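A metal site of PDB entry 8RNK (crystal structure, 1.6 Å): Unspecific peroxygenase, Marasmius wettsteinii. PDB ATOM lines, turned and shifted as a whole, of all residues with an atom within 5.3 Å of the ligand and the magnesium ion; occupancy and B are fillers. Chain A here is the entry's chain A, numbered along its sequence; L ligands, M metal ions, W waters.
N of His 90 sits close to O1 of the ligand (2.8 Å).
A ring nitrogen (NE2) of His 90 sits close to an oxygen (O2) of the ligand, at 3.3 Å.
SG of Cys 21 binds FE1 of the ligand, 2.3 Å away.
The backbone NH (N) of Ser 95 is in hydrogen-bond range of an oxygen (O3) of the ligand (2.8 Å).
OG of Ser 95 sits at hydrogen-bond distance from O3 of the ligand, 2.6 Å away.
An oxygen (O4) of the ligand sits at hydrogen-bond distance from the backbone NH (N) of Leu 94 (2.7 Å).
The side-chain carboxylate (OE1) of Glu 89 lies within hydrogen-bond range of the side-chain amide nitrogen (ND2) of Asn 104.
A ring nitrogen (NE2) of His 90 lies within hydrogen-bond range of the side-chain carboxylate of Glu 161.
SG of Cys 21 lies close to N of Gly 23, 3.3 Å away.
The side-chain sulfur (SG) of Cys 21 lies close to the backbone NH (N) of Leu 24.
The side-chain hydroxyl (OG) of Ser 95 is in hydrogen-bond range of the guanidinium group (NH1) of Arg 96.
The backbone carbonyl oxygen of Gly 23 is in hydrogen-bond range of the side-chain hydroxyl of Tyr 53, at 2.7 Å.
CG of Pro 20 touches C10 of the ligand (3.7 Å).
Pro 22 touches the ligand.
Gly 23 touches the ligand (CA to C22, 3.6 Å).
CD1 of Leu 24 touches C15 of the ligand, at 3.7 Å.
CG2 of Ile 45 touches C18 of the ligand, 3.8 Å away.
CD2 of Tyr 53 touches C24 of the ligand (3.9 Å).
O of Leu 60 touches C19 of the ligand, at 3.5 Å.
CB of Ala 63 touches C19 of the ligand, 3.3 Å away.
N of Gly 64 touches C19 of the ligand, at 3.2 Å.
O of Leu 82 touches C9 of the ligand, 3.4 Å away.
CG2 of Ile 88 touches C9 of the ligand, at 3.5 Å.
Arg 96 touches the ligand.
Glu 161 touches the ligand.
CD2 of Phe 164 touches C23 of the ligand (3.5 Å).
CG2 of Val 168 touches C26 of the ligand, at 3.9 Å.
Phe 187 touches the ligand (CZ to C26, 3.4 Å).
CZ of Phe 188 touches C31 of the ligand, 3.8 Å away.
23 residues have an atom within 4 Å of the ligand: Pro 20, Cys 21, Pro 22, Gly 23, Leu 24, Ile 45, Tyr 53, Leu 60, Ala 63, Gly 64, Leu 82, Ile 88, Glu 89, His 90, Ser 93, Leu 94, Ser 95, Arg 96, Glu 161, Phe 164, Val 168, Phe 187 and Phe 188.
The nearest printed residue that does not touch the magnesium ion is Asp 91 (4.3 Å).
The magnesium ion is bound by OE2 of Glu 89 (2.1 Å), water W1 (2.1 Å), water W4 (2.1 Å), O of His 90 (2.1 Å), OG of Ser 93 (2.1 Å) and O1 of the ligand (2.1 Å).
The magnesium ion has six donor atoms within binding distance.
Water W3 lies within hydrogen-bond range of O4 of the ligand (2.6 Å) and OE1 of Glu 161 (2.7 Å).
Water W2 bridges O of Pro 20 and O2 of the ligand.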
ATOM      1  N   PRO A  20      25.136  13.234 -23.521  1.00  0.00           N
ATOM      2  CA  PRO A  20      24.392  12.545 -22.469  1.00  0.00           C
ATOM      3  C   PRO A  20      25.000  12.641 -21.082  1.00  0.00           C
ATOM      4  O   PRO A  20      24.459  12.072 -20.140  1.00  0.00           O
ATOM      5  CB  PRO A  20      24.427  11.109 -23.028  1.00  0.00           C
ATOM      6  CG  PRO A  20      25.831  11.011 -23.592  1.00  0.00           C
ATOM      7  CD  PRO A  20      26.045  12.352 -24.270  1.00  0.00           C
ATOM      8  N   CYS A  21      26.145  13.332 -20.983  1.00  0.00           N
ATOM      9  CA  CYS A  21      26.891  13.440 -19.734  1.00  0.00           C
ATOM     10  C   CYS A  21      26.638  14.800 -19.072  1.00  0.00           C
ATOM     11  O   CYS A  21      27.109  15.813 -19.577  1.00  0.00           O
ATOM     12  CB  CYS A  21      28.372  13.253 -19.978  1.00  0.00           C
ATOM     13  SG  CYS A  21      29.353  13.466 -18.472  1.00  0.00           S
ATOM     14  N   PRO A  22      26.013  14.841 -17.879  1.00  0.00           N
ATOM     15  CA  PRO A  22      25.864  16.106 -17.160  1.00  0.00           C
ATOM     16  C   PRO A  22      27.206  16.685 -16.704  1.00  0.00           C
ATOM     17  O   PRO A  22      27.330  17.903 -16.556  1.00  0.00           O
ATOM     18  CB  PRO A  22      24.977  15.733 -15.969  1.00  0.00           C
ATOM     19  CG  PRO A  22      25.278  14.279 -15.732  1.00  0.00           C
ATOM     20  CD  PRO A  22      25.427  13.720 -17.138  1.00  0.00           C
ATOM     21  N   GLY A  23      28.199  15.827 -16.466  1.00  0.00           N
ATOM     22  CA  GLY A  23      29.499  16.323 -16.025  1.00  0.00           C
ATOM     23  C   GLY A  23      30.135  17.232 -17.054  1.00  0.00           C
ATOM     24  O   GLY A  23      30.553  18.364 -16.765  1.00  0.00           O
ATOM     25  N   LEU A  24      30.266  16.717 -18.279  1.00  0.00           N
ATOM     26  CA  LEU A  24      30.901  17.458 -19.356  1.00  0.00           C
ATOM     27  C   LEU A  24      30.001  18.597 -19.802  1.00  0.00           C
ATOM     28  O   LEU A  24      30.493  19.670 -20.125  1.00  0.00           O
ATOM     29  CB  LEU A  24      31.232  16.525 -20.514  1.00  0.00           C
ATOM     30  CG  LEU A  24      32.220  15.414 -20.193  1.00  0.00           C
ATOM     31  CD1 LEU A  24      32.451  14.577 -21.422  1.00  0.00           C
ATOM     32  CD2 LEU A  24      33.530  15.958 -19.638  1.00  0.00           C
ATOM     33  N   LEU A  27      30.471  21.481 -17.454  1.00  0.00           N
ATOM     34  CA  LEU A  27      31.739  22.146 -17.687  1.00  0.00           C
ATOM     35  C   LEU A  27      31.639  23.078 -18.905  1.00  0.00           C
ATOM     36  O   LEU A  27      32.172  24.195 -18.855  1.00  0.00           O
ATOM     37  CB  LEU A  27      32.869  21.123 -17.845  1.00  0.00           C
ATOM     38  CG  LEU A  27      33.246  20.362 -16.566  1.00  0.00           C
ATOM     39  CD1 LEU A  27      34.198  19.235 -16.897  1.00  0.00           C
ATOM     40  CD2 LEU A  27      33.836  21.280 -15.499  1.00  0.00           C
ATOM     41  N   ILE A  45      39.569  17.938 -21.581  1.00  0.00           N
ATOM     42  CA  ILE A  45      38.727  17.330 -20.557  1.00  0.00           C
ATOM     43  C   ILE A  45      39.472  17.204 -19.224  1.00  0.00           C
ATOM     44  O   ILE A  45      38.904  17.463 -18.156  1.00  0.00           O
ATOM     45  CB  ILE A  45      38.194  15.964 -21.052  1.00  0.00           C
ATOM     46  CG1 ILE A  45      37.230  16.140 -22.216  1.00  0.00           C
ATOM     47  CG2 ILE A  45      37.560  15.226 -19.902  1.00  0.00           C
ATOM     48  CD1 ILE A  45      36.858  14.872 -22.931  1.00  0.00           C
ATOM     49  N   TYR A  53      36.041  20.522 -10.954  1.00  0.00           N
ATOM     50  CA  TYR A  53      35.526  19.542 -10.022  1.00  0.00           C
ATOM     51  C   TYR A  53      36.603  18.927  -9.127  1.00  0.00           C
ATOM     52  O   TYR A  53      36.261  18.202  -8.193  1.00  0.00           O
ATOM     53  CB  TYR A  53      34.876  18.378 -10.786  1.00  0.00           C
ATOM     54  CG  TYR A  53      33.732  18.682 -11.716  1.00  0.00           C
ATOM     55  CD1 TYR A  53      32.736  19.582 -11.381  1.00  0.00           C
ATOM     56  CD2 TYR A  53      33.584  17.998 -12.916  1.00  0.00           C
ATOM     57  CE1 TYR A  53      31.659  19.824 -12.223  1.00  0.00           C
ATOM     58  CE2 TYR A  53      32.494  18.212 -13.755  1.00  0.00           C
ATOM     59  CZ  TYR A  53      31.530  19.136 -13.412  1.00  0.00           C
ATOM     60  OH  TYR A  53      30.462  19.366 -14.239  1.00  0.00           O
ATOM     61  N   VAL A  55      38.504  16.661 -10.254  1.00  0.00           N
ATOM     62  CA  VAL A  55      38.650  15.288 -10.714  1.00  0.00           C
ATOM     63  C   VAL A  55      40.002  15.140 -11.401  1.00  0.00           C
ATOM     64  O   VAL A  55      40.388  15.996 -12.201  1.00  0.00           O
ATOM     65  CB  VAL A  55      37.479  14.882 -11.636  1.00  0.00           C
ATOM     66  CG1 VAL A  55      37.711  13.509 -12.238  1.00  0.00           C
ATOM     67  CG2 VAL A  55      36.163  14.916 -10.900  1.00  0.00           C
ATOM     68  N   ILE A  59      41.136   9.052 -14.005  1.00  0.00           N
ATOM     69  CA  ILE A  59      39.834   8.635 -14.513  1.00  0.00           C
ATOM     70  C   ILE A  59      39.545   9.374 -15.819  1.00  0.00           C
ATOM     71  O   ILE A  59      38.920   8.799 -16.701  1.00  0.00           O
ATOM     72  CB  ILE A  59      38.706   8.808 -13.468  1.00  0.00           C
ATOM     73  CG1 ILE A  59      37.384   8.220 -13.964  1.00  0.00           C
ATOM     74  CG2 ILE A  59      38.559  10.248 -13.054  1.00  0.00           C
ATOM     75  CD1 ILE A  59      36.340   8.028 -12.886  1.00  0.00           C
ATOM     76  N   LEU A  60      39.971  10.622 -15.962  1.00  0.00           N
ATOM     77  CA  LEU A  60      39.577  11.404 -17.127  1.00  0.00           C
ATOM     78  C   LEU A  60      40.320  10.971 -18.375  1.00  0.00           C
ATOM     79  O   LEU A  60      39.771  11.049 -19.470  1.00  0.00           O
ATOM     80  CB  LEU A  60      39.731  12.909 -16.850  1.00  0.00           C
ATOM     81  CG  LEU A  60      38.824  13.416 -15.745  1.00  0.00           C
ATOM     82  CD1 LEU A  60      39.082  14.883 -15.472  1.00  0.00           C
ATOM     83  CD2 LEU A  60      37.346  13.195 -16.093  1.00  0.00           C
ATOM     84  N   ALA A  63      38.536   7.347 -19.218  1.00  0.00           N
ATOM     85  CA  ALA A  63      37.213   7.562 -19.793  1.00  0.00           C
ATOM     86  C   ALA A  63      37.291   8.418 -21.061  1.00  0.00           C
ATOM     87  O   ALA A  63      36.613   8.141 -22.063  1.00  0.00           O
ATOM     88  CB  ALA A  63      36.326   8.194 -18.747  1.00  0.00           C
ATOM     89  N   GLY A  64      38.116   9.468 -21.037  1.00  0.00           N
ATOM     90  CA  GLY A  64      38.241  10.372 -22.154  1.00  0.00           C
ATOM     91  C   GLY A  64      38.634   9.667 -23.449  1.00  0.00           C
ATOM     92  O   GLY A  64      38.082   9.955 -24.508  1.00  0.00           O
ATOM     93  N   GLY A  67      35.863   7.806 -24.811  1.00  0.00           N
ATOM     94  CA  GLY A  67      34.919   8.737 -25.432  1.00  0.00           C
ATOM     95  C   GLY A  67      35.360   9.205 -26.807  1.00  0.00           C
ATOM     96  O   GLY A  67      34.556   9.466 -27.679  1.00  0.00           O
ATOM     97  N   LEU A  82      29.131  11.642 -27.917  1.00  0.00           N
ATOM     98  CA  LEU A  82      29.160  10.683 -26.816  1.00  0.00           C
ATOM     99  C   LEU A  82      27.842   9.931 -26.643  1.00  0.00           C
ATOM    100  O   LEU A  82      27.785   8.962 -25.878  1.00  0.00           O
ATOM    101  CB  LEU A  82      29.505  11.447 -25.535  1.00  0.00           C
ATOM    102  CG  LEU A  82      30.918  11.993 -25.451  1.00  0.00           C
ATOM    103  CD1 LEU A  82      31.090  12.851 -24.205  1.00  0.00           C
ATOM    104  CD2 LEU A  82      31.921  10.874 -25.460  1.00  0.00           C
ATOM    105  N   ILE A  88      30.293   4.285 -24.483  1.00  0.00           N
ATOM    106  CA  ILE A  88      30.016   4.520 -23.076  1.00  0.00           C
ATOM    107  C   ILE A  88      28.502   4.547 -22.821  1.00  0.00           C
ATOM    108  O   ILE A  88      28.025   3.936 -21.869  1.00  0.00           O
ATOM    109  CB  ILE A  88      30.697   5.810 -22.586  1.00  0.00           C
ATOM    110  CG1 ILE A  88      32.219   5.704 -22.693  1.00  0.00           C
ATOM    111  CG2 ILE A  88      30.293   6.125 -21.162  1.00  0.00           C
ATOM    112  CD1 ILE A  88      32.900   7.041 -22.547  1.00  0.00           C
ATOM    113  N   GLU A  89      27.754   5.226 -23.688  1.00  0.00           N
ATOM    114  CA  GLU A  89      26.323   5.407 -23.478  1.00  0.00           C
ATOM    115  C   GLU A  89      25.643   4.041 -23.351  1.00  0.00           C
ATOM    116  O   GLU A  89      25.950   3.109 -24.101  1.00  0.00           O
ATOM    117  CB  GLU A  89      25.711   6.261 -24.580  1.00  0.00           C
ATOM    118  CG  GLU A  89      24.320   6.757 -24.230  1.00  0.00           C
ATOM    119  CD  GLU A  89      23.227   5.715 -24.380  1.00  0.00           C
ATOM    120  OE1 GLU A  89      23.279   4.998 -25.390  1.00  0.00           O
ATOM    121  OE2 GLU A  89      22.328   5.698 -23.542  1.00  0.00           O
ATOM    122  N   HIS A  90      24.756   3.946 -22.379  1.00  0.00           N
ATOM    123  CA  HIS A  90      24.148   2.682 -21.985  1.00  0.00           C
ATOM    124  C   HIS A  90      22.673   2.877 -21.645  1.00  0.00           C
ATOM    125  O   HIS A  90      22.214   3.959 -21.297  1.00  0.00           O
ATOM    126  CB  HIS A  90      24.883   2.081 -20.774  1.00  0.00           C
ATOM    127  CG  HIS A  90      25.045   3.058 -19.666  1.00  0.00           C
ATOM    128  ND1 HIS A  90      23.996   3.384 -18.848  1.00  0.00           N
ATOM    129  CD2 HIS A  90      26.074   3.850 -19.273  1.00  0.00           C
ATOM    130  CE1 HIS A  90      24.373   4.343 -18.010  1.00  0.00           C
ATOM    131  NE2 HIS A  90      25.629   4.633 -18.243  1.00  0.00           N
ATOM    132  N   ASP A  91      21.970   1.747 -21.585  1.00  0.00           N
ATOM    133  CA  ASP A  91      20.614   1.699 -21.072  1.00  0.00           C
ATOM    134  C   ASP A  91      20.613   1.906 -19.561  1.00  0.00           C
ATOM    135  O   ASP A  91      21.663   1.822 -18.923  1.00  0.00           O
ATOM    136  CB  ASP A  91      19.998   0.352 -21.423  1.00  0.00           C
ATOM    137  CG  ASP A  91      19.891   0.131 -22.914  1.00  0.00           C
ATOM    138  OD1 ASP A  91      19.759   1.130 -23.656  1.00  0.00           O
ATOM    139  OD2 ASP A  91      19.921  -1.052 -23.340  1.00  0.00           O
ATOM    140  N   SER A  93      20.058   4.593 -17.845  1.00  0.00           N
ATOM    141  CA  SER A  93      20.608   5.858 -17.383  1.00  0.00           C
ATOM    142  C   SER A  93      19.718   6.454 -16.283  1.00  0.00           C
ATOM    143  O   SER A  93      18.556   6.110 -16.172  1.00  0.00           O
ATOM    144  CB  SER A  93      20.736   6.815 -18.540  1.00  0.00           C
ATOM    145  OG  SER A  93      21.730   6.376 -19.456  1.00  0.00           O
ATOM    146  N   LEU A  94      20.258   7.436 -15.547  1.00  0.00           N
ATOM    147  CA  LEU A  94      19.577   8.066 -14.431  1.00  0.00           C
ATOM    148  C   LEU A  94      18.638   9.164 -14.909  1.00  0.00           C
ATOM    149  O   LEU A  94      17.726   9.526 -14.162  1.00  0.00           O
ATOM    150  CB  LEU A  94      20.629   8.687 -13.517  1.00  0.00           C
ATOM    151  CG  LEU A  94      21.611   7.716 -12.869  1.00  0.00           C
ATOM    152  CD1 LEU A  94      22.828   8.459 -12.319  1.00  0.00           C
ATOM    153  CD2 LEU A  94      20.939   6.891 -11.798  1.00  0.00           C
ATOM    154  N   SER A  95      18.908   9.733 -16.086  1.00  0.00           N
ATOM    155  CA  SER A  95      18.217  10.956 -16.505  1.00  0.00           C
ATOM    156  C   SER A  95      17.900  10.976 -17.999  1.00  0.00           C
ATOM    157  O   SER A  95      17.375  11.973 -18.481  1.00  0.00           O
ATOM    158  CB  SER A  95      19.029  12.193 -16.102  1.00  0.00           C
ATOM    159  OG  SER A  95      20.245  12.297 -16.826  1.00  0.00           O
ATOM    160  N   ARG A  96      18.234   9.904 -18.725  1.00  0.00           N
ATOM    161  CA  ARG A  96      17.986   9.782 -20.150  1.00  0.00           C
ATOM    162  C   ARG A  96      17.194   8.495 -20.394  1.00  0.00           C
ATOM    163  O   ARG A  96      17.238   7.583 -19.562  1.00  0.00           O
ATOM    164  CB  ARG A  96      19.276   9.710 -20.974  1.00  0.00           C
ATOM    165  CG  ARG A  96      19.899  11.054 -21.374  1.00  0.00           C
ATOM    166  CD  ARG A  96      20.238  11.978 -20.249  1.00  0.00           C
ATOM    167  NE  ARG A  96      20.980  13.127 -20.733  1.00  0.00           N
ATOM    168  CZ  ARG A  96      21.370  14.188 -20.014  1.00  0.00           C
ATOM    169  NH1 ARG A  96      21.135  14.263 -18.718  1.00  0.00           N
ATOM    170  NH2 ARG A  96      21.974  15.190 -20.623  1.00  0.00           N
ATOM    171  N   GLU A  97      16.534   8.425 -21.558  1.00  0.00           N
ATOM    172  CA  GLU A  97      15.800   7.224 -21.944  1.00  0.00           C
ATOM    173  C   GLU A  97      16.757   6.281 -22.666  1.00  0.00           C
ATOM    174  O   GLU A  97      17.774   6.715 -23.197  1.00  0.00           O
ATOM    175  CB  GLU A  97      14.622   7.594 -22.862  1.00  0.00           C
ATOM    176  CG  GLU A  97      13.637   8.551 -22.217  1.00  0.00           C
ATOM    177  CD  GLU A  97      12.531   9.012 -23.150  1.00  0.00           C
ATOM    178  OE1 GLU A  97      12.818   9.283 -24.331  1.00  0.00           O
ATOM    179  OE2 GLU A  97      11.368   9.099 -22.676  1.00  0.00           O
ATOM    180  N   ASN A 104      18.168   9.091 -25.940  1.00  0.00           N
ATOM    181  CA  ASN A 104      19.291   8.716 -25.084  1.00  0.00           C
ATOM    182  C   ASN A 104      20.244   9.875 -24.852  1.00  0.00           C
ATOM    183  O   ASN A 104      21.322   9.644 -24.313  1.00  0.00           O
ATOM    184  CB  ASN A 104      20.062   7.523 -25.651  1.00  0.00           C
ATOM    185  CG  ASN A 104      20.939   7.856 -26.832  1.00  0.00           C
ATOM    186  OD1 ASN A 104      20.728   8.860 -27.496  1.00  0.00           O
ATOM    187  ND2 ASN A 104      21.957   7.045 -27.077  1.00  0.00           N
ATOM    188  N   GLU A 161      29.181   6.428 -12.629  1.00  0.00           N
ATOM    189  CA  GLU A 161      28.440   7.669 -12.841  1.00  0.00           C
ATOM    190  C   GLU A 161      27.733   8.102 -11.556  1.00  0.00           C
ATOM    191  O   GLU A 161      27.719   9.282 -11.214  1.00  0.00           O
ATOM    192  CB  GLU A 161      27.508   7.485 -14.031  1.00  0.00           C
ATOM    193  CG  GLU A 161      28.303   7.426 -15.329  1.00  0.00           C
ATOM    194  CD  GLU A 161      27.666   6.745 -16.533  1.00  0.00           C
ATOM    195  OE1 GLU A 161      26.580   6.234 -16.412  1.00  0.00           O
ATOM    196  OE2 GLU A 161      28.321   6.807 -17.590  1.00  0.00           O
ATOM    197  N   SER A 162      27.138   7.147 -10.833  1.00  0.00           N
ATOM    198  CA  SER A 162      26.552   7.456  -9.533  1.00  0.00           C
ATOM    199  C   SER A 162      27.633   7.943  -8.558  1.00  0.00           C
ATOM    200  O   SER A 162      27.418   8.934  -7.843  1.00  0.00           O
ATOM    201  CB  SER A 162      25.801   6.278  -8.951  1.00  0.00           C
ATOM    202  OG  SER A 162      24.675   5.945  -9.765  1.00  0.00           O
ATOM    203  N   PHE A 164      30.292   9.543  -9.363  1.00  0.00           N
ATOM    204  CA  PHE A 164      30.614  10.891  -9.794  1.00  0.00           C
ATOM    205  C   PHE A 164      29.652  11.897  -9.177  1.00  0.00           C
ATOM    206  O   PHE A 164      30.093  12.928  -8.646  1.00  0.00           O
ATOM    207  CB  PHE A 164      30.625  11.021 -11.322  1.00  0.00           C
ATOM    208  CG  PHE A 164      31.963  10.872 -11.976  1.00  0.00           C
ATOM    209  CD1 PHE A 164      33.081  11.479 -11.426  1.00  0.00           C
ATOM    210  CD2 PHE A 164      32.060  10.296 -13.241  1.00  0.00           C
ATOM    211  CE1 PHE A 164      34.312  11.398 -12.067  1.00  0.00           C
ATOM    212  CE2 PHE A 164      33.299  10.223 -13.873  1.00  0.00           C
ATOM    213  CZ  PHE A 164      34.408  10.778 -13.292  1.00  0.00           C
ATOM    214  N   TYR A 165      28.331  11.664  -9.278  1.00  0.00           N
ATOM    215  CA  TYR A 165      27.424  12.694  -8.778  1.00  0.00           C
ATOM    216  C   TYR A 165      27.505  12.805  -7.258  1.00  0.00           C
ATOM    217  O   TYR A 165      27.437  13.923  -6.735  1.00  0.00           O
ATOM    218  CB  TYR A 165      25.984  12.581  -9.336  1.00  0.00           C
ATOM    219  CG  TYR A 165      25.060  11.571  -8.712  1.00  0.00           C
ATOM    220  CD1 TYR A 165      24.555  11.746  -7.434  1.00  0.00           C
ATOM    221  CD2 TYR A 165      24.651  10.461  -9.416  1.00  0.00           C
ATOM    222  CE1 TYR A 165      23.665  10.858  -6.867  1.00  0.00           C
ATOM    223  CE2 TYR A 165      23.771   9.533  -8.864  1.00  0.00           C
ATOM    224  CZ  TYR A 165      23.270   9.737  -7.583  1.00  0.00           C
ATOM    225  OH  TYR A 165      22.426   8.775  -7.063  1.00  0.00           O
ATOM    226  N   VAL A 168      31.401  14.664  -6.827  1.00  0.00           N
ATOM    227  CA  VAL A 168      31.684  15.972  -7.399  1.00  0.00           C
ATOM    228  C   VAL A 168      30.741  17.031  -6.832  1.00  0.00           C
ATOM    229  O   VAL A 168      31.136  18.204  -6.690  1.00  0.00           O
ATOM    230  CB  VAL A 168      31.640  15.878  -8.940  1.00  0.00           C
ATOM    231  CG1 VAL A 168      31.609  17.218  -9.601  1.00  0.00           C
ATOM    232  CG2 VAL A 168      32.773  15.029  -9.489  1.00  0.00           C
ATOM    233  N   PHE A 187      22.566  20.062 -10.791  1.00  0.00           N
ATOM    234  CA  PHE A 187      23.536  19.471 -11.687  1.00  0.00           C
ATOM    235  C   PHE A 187      22.842  18.764 -12.846  1.00  0.00           C
ATOM    236  O   PHE A 187      23.169  19.004 -14.000  1.00  0.00           O
ATOM    237  CB  PHE A 187      24.461  18.582 -10.850  1.00  0.00           C
ATOM    238  CG  PHE A 187      25.496  17.812 -11.609  1.00  0.00           C
ATOM    239  CD1 PHE A 187      26.575  18.454 -12.185  1.00  0.00           C
ATOM    240  CD2 PHE A 187      25.402  16.433 -11.727  1.00  0.00           C
ATOM    241  CE1 PHE A 187      27.544  17.742 -12.888  1.00  0.00           C
ATOM    242  CE2 PHE A 187      26.383  15.727 -12.413  1.00  0.00           C
ATOM    243  CZ  PHE A 187      27.444  16.383 -12.998  1.00  0.00           C
ATOM    244  N   PHE A 188      21.847  17.913 -12.543  1.00  0.00           N
ATOM    245  CA  PHE A 188      21.175  17.160 -13.593  1.00  0.00           C
ATOM    246  C   PHE A 188      20.168  18.026 -14.369  1.00  0.00           C
ATOM    247  O   PHE A 188      20.128  18.000 -15.593  1.00  0.00           O
ATOM    248  CB  PHE A 188      20.429  15.966 -12.968  1.00  0.00           C
ATOM    249  CG  PHE A 188      21.265  14.720 -12.760  1.00  0.00           C
ATOM    250  CD1 PHE A 188      21.452  13.808 -13.793  1.00  0.00           C
ATOM    251  CD2 PHE A 188      21.874  14.457 -11.550  1.00  0.00           C
ATOM    252  CE1 PHE A 188      22.206  12.659 -13.594  1.00  0.00           C
ATOM    253  CE2 PHE A 188      22.636  13.307 -11.358  1.00  0.00           C
ATOM    254  CZ  PHE A 188      22.785  12.400 -12.376  1.00  0.00           C
HETATM  255  C1  LIG L   1      27.043   9.868 -18.045  1.00  0.00           C
HETATM  256  C2  LIG L   1      31.016  10.265 -20.769  1.00  0.00           C
HETATM  257  C3  LIG L   1      33.182  12.710 -17.216  1.00  0.00           C
HETATM  258  C4  LIG L   1      29.154  12.471 -14.542  1.00  0.00           C
HETATM  259  C5  LIG L   1      27.908   9.833 -19.103  1.00  0.00           C
HETATM  260  C6  LIG L   1      27.620   9.294 -20.385  1.00  0.00           C
HETATM  261  C7  LIG L   1      28.709   9.383 -21.151  1.00  0.00           C
HETATM  262  C8  LIG L   1      29.720  10.013 -20.354  1.00  0.00           C
HETATM  263  C9  LIG L   1      28.835   8.974 -22.594  1.00  0.00           C
HETATM  264  C10 LIG L   1      26.290   8.717 -20.788  1.00  0.00           C
HETATM  265  C11 LIG L   1      26.159   7.309 -20.192  1.00  0.00           C
HETATM  266  C12 LIG L   1      24.684   6.974 -20.043  1.00  0.00           C
HETATM  267  O1  LIG L   1      24.095   6.250 -20.921  1.00  0.00           O
HETATM  268  O2  LIG L   1      24.021   7.443 -19.072  1.00  0.00           O
HETATM  269  C13 LIG L   1      31.973  10.927 -20.002  1.00  0.00           C
HETATM  270  C14 LIG L   1      33.334  11.131 -20.459  1.00  0.00           C
HETATM  271  C15 LIG L   1      33.940  11.848 -19.447  1.00  0.00           C
HETATM  272  C16 LIG L   1      32.948  12.027 -18.382  1.00  0.00           C
HETATM  273  C17 LIG L   1      33.906  10.757 -21.788  1.00  0.00           C
HETATM  274  C18 LIG L   1      35.316  12.309 -19.174  1.00  0.00           C
HETATM  275  C19 LIG L   1      36.288  11.472 -19.394  1.00  0.00           C
HETATM  276  C20 LIG L   1      32.279  12.951 -16.209  1.00  0.00           C
HETATM  277  C21 LIG L   1      32.471  13.789 -15.091  1.00  0.00           C
HETATM  278  C22 LIG L   1      31.331  13.698 -14.328  1.00  0.00           C
HETATM  279  C23 LIG L   1      30.398  12.815 -14.977  1.00  0.00           C
HETATM  280  C24 LIG L   1      33.720  14.592 -14.768  1.00  0.00           C
HETATM  281  C25 LIG L   1      31.189  14.443 -13.045  1.00  0.00           C
HETATM  282  C26 LIG L   1      30.135  14.447 -12.258  1.00  0.00           C
HETATM  283  C27 LIG L   1      28.233  11.667 -15.291  1.00  0.00           C
HETATM  284  C28 LIG L   1      26.916  11.233 -14.755  1.00  0.00           C
HETATM  285  C29 LIG L   1      26.360  10.517 -15.764  1.00  0.00           C
HETATM  286  C30 LIG L   1      27.328  10.529 -16.856  1.00  0.00           C
HETATM  287  C31 LIG L   1      26.378  11.557 -13.386  1.00  0.00           C
HETATM  288  C32 LIG L   1      25.044   9.818 -15.702  1.00  0.00           C
HETATM  289  C33 LIG L   1      23.921  10.431 -16.505  1.00  0.00           C
HETATM  290  C34 LIG L   1      22.690   9.586 -16.459  1.00  0.00           C
HETATM  291  O3  LIG L   1      21.593  10.068 -16.832  1.00  0.00           O
HETATM  292  O4  LIG L   1      22.766   8.391 -16.088  1.00  0.00           O
HETATM  293  N1  LIG L   1      29.239  10.217 -19.098  1.00  0.00           N
HETATM  294  N2  LIG L   1      31.810  11.405 -18.764  1.00  0.00           N
HETATM  295  N3  LIG L   1      31.021  12.445 -16.143  1.00  0.00           N
HETATM  296  N4  LIG L   1      28.486  11.196 -16.539  1.00  0.00           N
HETATM  297 FE1  LIG L   1      30.023  11.422 -17.682  1.00  0.00          FE
HETATM  298 MG    MG M   1      22.060   6.061 -21.538  1.00  0.00          MG
HETATM  299  O   HOH W   1      19.997   5.877 -21.770  1.00  0.00           O
HETATM  300  O   HOH W   2      22.802   9.883 -20.008  1.00  0.00           O
HETATM  301  O   HOH W   3      24.080   6.212 -15.353  1.00  0.00           O
HETATM  302  O   HOH W   4      22.047   8.121 -21.993  1.00  0.00           O
